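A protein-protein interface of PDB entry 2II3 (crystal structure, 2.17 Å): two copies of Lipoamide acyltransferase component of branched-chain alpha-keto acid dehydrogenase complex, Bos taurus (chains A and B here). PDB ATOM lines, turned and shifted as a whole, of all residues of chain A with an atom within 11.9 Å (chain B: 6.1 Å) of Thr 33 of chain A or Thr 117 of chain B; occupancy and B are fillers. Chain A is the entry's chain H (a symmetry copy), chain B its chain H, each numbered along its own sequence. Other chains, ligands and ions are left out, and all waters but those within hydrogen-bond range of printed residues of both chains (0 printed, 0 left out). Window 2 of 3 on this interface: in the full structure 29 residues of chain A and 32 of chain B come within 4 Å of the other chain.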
ATOM      1  N   GLY A  29      37.803  28.536   1.089  1.00  0.00           N
ATOM      2  CA  GLY A  29      36.945  28.350   2.297  1.00  0.00           C
ATOM      3  C   GLY A  29      36.119  27.070   2.313  1.00  0.00           C
ATOM      4  O   GLY A  29      36.570  26.042   2.822  1.00  0.00           O
ATOM      5  N   LYS A  30      34.898  27.144   1.779  1.00  0.00           N
ATOM      6  CA  LYS A  30      33.942  26.022   1.792  1.00  0.00           C
ATOM      7  C   LYS A  30      33.296  25.872   0.414  1.00  0.00           C
ATOM      8  O   LYS A  30      33.455  26.752  -0.437  1.00  0.00           O
ATOM      9  CB  LYS A  30      32.836  26.274   2.826  1.00  0.00           C
ATOM     10  CG  LYS A  30      33.302  26.748   4.194  1.00  0.00           C
ATOM     11  CD  LYS A  30      33.661  25.580   5.118  1.00  0.00           C
ATOM     12  CE  LYS A  30      34.490  26.048   6.303  1.00  0.00           C
ATOM     13  NZ  LYS A  30      34.083  27.412   6.730  1.00  0.00           N
ATOM     14  N   ASP A  31      32.566  24.771   0.198  1.00  0.00           N
ATOM     15  CA  ASP A  31      31.837  24.564  -1.072  1.00  0.00           C
ATOM     16  C   ASP A  31      30.562  25.428  -1.149  1.00  0.00           C
ATOM     17  O   ASP A  31      29.853  25.588  -0.157  1.00  0.00           O
ATOM     18  CB  ASP A  31      31.517  23.072  -1.312  1.00  0.00           C
ATOM     19  CG  ASP A  31      32.778  22.201  -1.517  1.00  0.00           C
ATOM     20  OD1 ASP A  31      33.914  22.719  -1.564  1.00  0.00           O
ATOM     21  OD2 ASP A  31      32.619  20.972  -1.615  1.00  0.00           O
ATOM     22  N   ARG A  32      30.313  26.001  -2.325  1.00  0.00           N
ATOM     23  CA  ARG A  32      29.166  26.864  -2.588  1.00  0.00           C
ATOM     24  C   ARG A  32      28.426  26.320  -3.837  1.00  0.00           C
ATOM     25  O   ARG A  32      28.931  26.423  -4.954  1.00  0.00           O
ATOM     26  CB  ARG A  32      29.653  28.325  -2.794  1.00  0.00           C
ATOM     27  CG  ARG A  32      28.577  29.381  -3.150  1.00  0.00           C
ATOM     28  CD  ARG A  32      29.157  30.760  -3.604  1.00  0.00           C
ATOM     29  NE  ARG A  32      30.538  30.716  -4.128  1.00  0.00           N
ATOM     30  CZ  ARG A  32      30.915  30.949  -5.394  1.00  0.00           C
ATOM     31  NH1 ARG A  32      30.021  31.262  -6.341  1.00  0.00           N
ATOM     32  NH2 ARG A  32      32.215  30.871  -5.726  1.00  0.00           N
ATOM     33  N   THR A  33      27.264  25.692  -3.633  1.00  0.00           N
ATOM     34  CA  THR A  33      26.384  25.321  -4.748  1.00  0.00           C
ATOM     35  C   THR A  33      25.514  26.524  -5.149  1.00  0.00           C
ATOM     36  O   THR A  33      25.173  27.374  -4.318  1.00  0.00           O
ATOM     37  CB  THR A  33      25.477  24.111  -4.456  1.00  0.00           C
ATOM     38  OG1 THR A  33      26.222  23.081  -3.795  1.00  0.00           O
ATOM     39  CG2 THR A  33      24.897  23.560  -5.756  1.00  0.00           C
ATOM     40  N   GLU A  34      25.125  26.549  -6.414  1.00  0.00           N
ATOM     41  CA  GLU A  34      24.604  27.743  -7.045  1.00  0.00           C
ATOM     42  C   GLU A  34      23.780  27.338  -8.283  1.00  0.00           C
ATOM     43  O   GLU A  34      24.227  26.502  -9.088  1.00  0.00           O
ATOM     44  CB  GLU A  34      25.814  28.585  -7.442  1.00  0.00           C
ATOM     45  CG  GLU A  34      25.571  29.861  -8.181  1.00  0.00           C
ATOM     46  CD  GLU A  34      26.443  30.977  -7.636  1.00  0.00           C
ATOM     47  OE1 GLU A  34      27.163  31.588  -8.453  1.00  0.00           O
ATOM     48  OE2 GLU A  34      26.396  31.234  -6.394  1.00  0.00           O
ATOM     49  N   PRO A  35      22.560  27.904  -8.434  1.00  0.00           N
ATOM     50  CA  PRO A  35      21.812  27.620  -9.657  1.00  0.00           C
ATOM     51  C   PRO A  35      22.492  28.236 -10.851  1.00  0.00           C
ATOM     52  O   PRO A  35      23.169  29.258 -10.717  1.00  0.00           O
ATOM     53  CB  PRO A  35      20.453  28.306  -9.426  1.00  0.00           C
ATOM     54  CG  PRO A  35      20.389  28.541  -7.967  1.00  0.00           C
ATOM     55  CD  PRO A  35      21.803  28.791  -7.537  1.00  0.00           C
ATOM     56  N   VAL A  36      22.345  27.577 -11.997  1.00  0.00           N
ATOM     57  CA  VAL A  36      22.695  28.149 -13.287  1.00  0.00           C
ATOM     58  C   VAL A  36      21.423  28.841 -13.769  1.00  0.00           C
ATOM     59  O   VAL A  36      20.364  28.196 -13.923  1.00  0.00           O
ATOM     60  CB  VAL A  36      23.150  27.066 -14.314  1.00  0.00           C
ATOM     61  CG1 VAL A  36      23.561  27.718 -15.593  1.00  0.00           C
ATOM     62  CG2 VAL A  36      24.295  26.215 -13.770  1.00  0.00           C
ATOM     63  N   LYS A  37      21.499  30.149 -13.982  1.00  0.00           N
ATOM     64  CA  LYS A  37      20.272  30.913 -14.236  1.00  0.00           C
ATOM     65  C   LYS A  37      20.424  31.900 -15.368  1.00  0.00           C
ATOM     66  O   LYS A  37      21.543  32.247 -15.738  1.00  0.00           O
ATOM     67  CB  LYS A  37      19.826  31.671 -12.971  1.00  0.00           C
ATOM     68  CG  LYS A  37      19.025  30.867 -11.971  1.00  0.00           C
ATOM     69  CD  LYS A  37      18.360  31.812 -10.965  1.00  0.00           C
ATOM     70  CE  LYS A  37      18.225  31.197  -9.587  1.00  0.00           C
ATOM     71  NZ  LYS A  37      17.104  30.220  -9.448  1.00  0.00           N
ATOM     72  N   ASN B 106      37.466  24.503 -11.094  1.00  0.00           N
ATOM     73  CA  ASN B 106      37.476  23.549  -9.983  1.00  0.00           C
ATOM     74  C   ASN B 106      36.059  23.486  -9.412  1.00  0.00           C
ATOM     75  O   ASN B 106      35.784  23.971  -8.301  1.00  0.00           O
ATOM     76  CB  ASN B 106      38.446  24.036  -8.929  1.00  0.00           C
ATOM     77  CG  ASN B 106      38.957  22.907  -8.046  1.00  0.00           C
ATOM     78  OD1 ASN B 106      39.756  22.061  -8.475  1.00  0.00           O
ATOM     79  ND2 ASN B 106      38.486  22.894  -6.782  1.00  0.00           N
ATOM     80  N   ALA B 107      35.141  22.943 -10.192  1.00  0.00           N
ATOM     81  CA  ALA B 107      33.718  22.941  -9.904  1.00  0.00           C
ATOM     82  C   ALA B 107      33.133  21.698 -10.551  1.00  0.00           C
ATOM     83  O   ALA B 107      33.818  21.036 -11.367  1.00  0.00           O
ATOM     84  CB  ALA B 107      33.050  24.166 -10.479  1.00  0.00           C
ATOM     85  N   SER B 108      31.877  21.416 -10.194  1.00  0.00           N
ATOM     86  CA  SER B 108      31.050  20.328 -10.711  1.00  0.00           C
ATOM     87  C   SER B 108      29.671  20.861 -11.006  1.00  0.00           C
ATOM     88  O   SER B 108      29.264  21.866 -10.476  1.00  0.00           O
ATOM     89  CB  SER B 108      30.828  19.240  -9.640  1.00  0.00           C
ATOM     90  OG  SER B 108      32.009  18.498  -9.429  1.00  0.00           O
ATOM     91  N   VAL B 109      28.946  20.077 -11.784  1.00  0.00           N
ATOM     92  CA  VAL B 109      27.709  20.415 -12.413  1.00  0.00           C
ATOM     93  C   VAL B 109      26.874  19.157 -12.169  1.00  0.00           C
ATOM     94  O   VAL B 109      27.431  18.049 -12.176  1.00  0.00           O
ATOM     95  CB  VAL B 109      28.052  20.704 -13.912  1.00  0.00           C
ATOM     96  CG1 VAL B 109      27.267  19.883 -14.856  1.00  0.00           C
ATOM     97  CG2 VAL B 109      27.973  22.182 -14.182  1.00  0.00           C
ATOM     98  N   ASN B 115      22.778  23.224 -11.812  1.00  0.00           N
ATOM     99  CA  ASN B 115      23.402  23.767 -10.615  1.00  0.00           C
ATOM    100  C   ASN B 115      24.900  23.511 -10.665  1.00  0.00           C
ATOM    101  O   ASN B 115      25.339  22.455 -11.106  1.00  0.00           O
ATOM    102  CB  ASN B 115      22.791  23.166  -9.327  1.00  0.00           C
ATOM    103  CG  ASN B 115      21.274  23.315  -9.265  1.00  0.00           C
ATOM    104  OD1 ASN B 115      20.561  22.357  -9.527  1.00  0.00           O
ATOM    105  ND2 ASN B 115      20.782  24.522  -8.963  1.00  0.00           N
ATOM    106  N   ILE B 116      25.665  24.495 -10.220  1.00  0.00           N
ATOM    107  CA  ILE B 116      27.096  24.405 -10.138  1.00  0.00           C
ATOM    108  C   ILE B 116      27.565  24.417  -8.664  1.00  0.00           C
ATOM    109  O   ILE B 116      27.156  25.292  -7.880  1.00  0.00           O
ATOM    110  CB  ILE B 116      27.753  25.566 -10.905  1.00  0.00           C
ATOM    111  CG1 ILE B 116      29.263  25.398 -10.880  1.00  0.00           C
ATOM    112  CG2 ILE B 116      27.343  26.894 -10.282  1.00  0.00           C
ATOM    113  CD1 ILE B 116      29.914  26.090 -11.928  1.00  0.00           C
ATOM    114  N   THR B 117      28.398  23.438  -8.302  1.00  0.00           N
ATOM    115  CA  THR B 117      29.068  23.409  -7.010  1.00  0.00           C
ATOM    116  C   THR B 117      30.524  23.827  -7.166  1.00  0.00           C
ATOM    117  O   THR B 117      31.336  23.131  -7.769  1.00  0.00           O
ATOM    118  CB  THR B 117      29.003  22.022  -6.388  1.00  0.00           C
ATOM    119  OG1 THR B 117      27.622  21.614  -6.286  1.00  0.00           O
ATOM    120  CG2 THR B 117      29.664  22.008  -4.981  1.00  0.00           C
ATOM    121  N   TYR B 118      30.829  25.014  -6.674  1.00  0.00           N
ATOM    122  CA  TYR B 118      32.181  25.512  -6.573  1.00  0.00           C
ATOM    123  C   TYR B 118      32.844  24.735  -5.435  1.00  0.00           C
ATOM    124  O   TYR B 118      32.328  24.693  -4.347  1.00  0.00           O
ATOM    125  CB  TYR B 118      32.144  27.009  -6.279  1.00  0.00           C
ATOM    126  CG  TYR B 118      31.663  27.770  -7.486  1.00  0.00           C
ATOM    127  CD1 TYR B 118      30.318  28.091  -7.642  1.00  0.00           C
ATOM    128  CD2 TYR B 118      32.553  28.169  -8.470  1.00  0.00           C
ATOM    129  CE1 TYR B 118      29.882  28.780  -8.764  1.00  0.00           C
ATOM    130  CE2 TYR B 118      32.136  28.842  -9.590  1.00  0.00           C
ATOM    131  CZ  TYR B 118      30.800  29.146  -9.740  1.00  0.00           C
ATOM    132  OH  TYR B 118      30.385  29.829 -10.868  1.00  0.00           O
ATOM    133  N   LYS B 119      33.982  24.107  -5.724  1.00  0.00           N
ATOM    134  CA  LYS B 119      34.679  23.274  -4.758  1.00  0.00           C
ATOM    135  C   LYS B 119      35.875  24.066  -4.296  1.00  0.00           C
ATOM    136  O   LYS B 119      36.611  24.639  -5.126  1.00  0.00           O
ATOM    137  CB  LYS B 119      35.077  21.946  -5.411  1.00  0.00           C
ATOM    138  CG  LYS B 119      33.879  21.273  -6.101  1.00  0.00           C
ATOM    139  CD  LYS B 119      33.769  19.806  -5.833  1.00  0.00           C
ATOM    140  CE  LYS B 119      32.417  19.299  -6.301  1.00  0.00           C
ATOM    141  NZ  LYS B 119      32.411  17.900  -6.846  1.00  0.00           N
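No position is printed for both chains.
Gly 29 of chain A touches none of the printed residues of chain B.
Of the printed residues of chain B, Asp 31 of chain A touches Tyr 118 and Lys 119.
Printed residues of chain B within 4 Å of Arg 32 of chain A: Ile 116, Thr 117 and Tyr 118.
Thr 33 of chain A touches just these residues of chain B: Ile 116 (3.2 Å) and Thr 117 (3.2 Å).
Printed residues of chain B within 4 Å of Pro 35 of chain A: Asn 115 (3.3 Å).
Printed residues of chain B within 4 Å of Val 36 of chain A: Asn 115 (3.9 Å).
No residue of chain A comes within 4 Å of Ser 108 of chain B.
No residue of chain A comes within 4 Å of Val 109 of chain B.
Ile 116 of chain B touches three residues of chain A.
Of chain A, only Arg 32 and Thr 33 come within 4 Å of Thr 117 of chain B.
Of chain A, only Asp 31 (3.3 Å), Arg 32 (2.9 Å) and Glu 34 (3.9 Å) come within 4 Å of Tyr 118 of chain B.
Lys 119 of chain B touches one residue of chain A.
The nearest residue of chain B that does not touch Thr 33 of chain A is Asn 115 of chain B (4.2 Å).
The nearest printed residue of chain B that does not touch Asp 31 of chain A is Thr 117 of chain B (4.2 Å).
Among the printed residues, pairs that only touch across the chains: Asp 31 of chain A with Tyr 118 of chain B (3.3 Å), Asp 31 of chain A with Lys 119 of chain B (3.3 Å), Arg 32 of chain A with Ile 116 of chain B (3.6 Å), Arg 32 of chain A with Thr 117 of chain B (3.7 Å), Thr 33 of chain A with Ile 116 of chain B (3.2 Å), Glu 34 of chain A with Asn 115 of chain B (3.2 Å), Glu 34 of chain A with Tyr 118 of chain B (3.9 Å), Pro 35 of chain A with Asn 115 of chain B (3.3 Å) and Val 36 of chain A with Asn 115 of chain B (3.9 Å).
Printed residues of chain B that touch a printed residue of chain A: Asn 115, Ile 116, Thr 117, Tyr 118 and Lys 119.
Hydrophobic or aromatic side chains of chain B that line the printed part of chain A: Ile 116 and Tyr 118.
Of the 9 printed residues of chain A, 6 touch a printed residue of chain B.
Printed residues of chain A that touch a printed residue of chain B: Asp 31, Arg 32, Thr 33, Glu 34, Pro 35 and Val 36.
Hydrophobic or aromatic side chains of chain A that line the printed part of chain B: Pro 35 and Val 36.
Among the printed residues, 12 pairs touch across the chains.
Among the printed residues, no Asp or Glu carboxylate lies within 4 Å of a Lys or Arg side-chain nitrogen of the other chain.
O of Arg 32 of chain A is in hydrogen-bond range of N of Tyr 118 of chain B, at 2.9 Å.
The backbone NH (N) of Ile 116 of chain B sits at hydrogen-bond distance from the backbone carbonyl oxygen (O) of Glu 34 of chain A, at 2.7 Å.
OG1 of Thr 33 of chain A sits at hydrogen-bond distance from OG1 of Thr 117 of chain B (3.2 Å).
The side-chain carboxylate (OE1) of Glu 34 of chain A lies within salt-bridge range of the guanidinium group (NH1) of Arg 32 of chain A.
The side-chain amide nitrogen (ND2) of Asn 106 of chain B sits at hydrogen-bond distance from the backbone carbonyl oxygen (O) of Lys 119 of chain B (3.1 Å).
N of Thr 117 of chain B is in hydrogen-bond range of O of Ser 108 of chain B (2.8 Å).
The side-chain hydroxyl (OG) of Ser 108 of chain B sits at hydrogen-bond distance from the side-chain amino group (NZ) of Lys 119 of chain B, 2.7 Å away.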
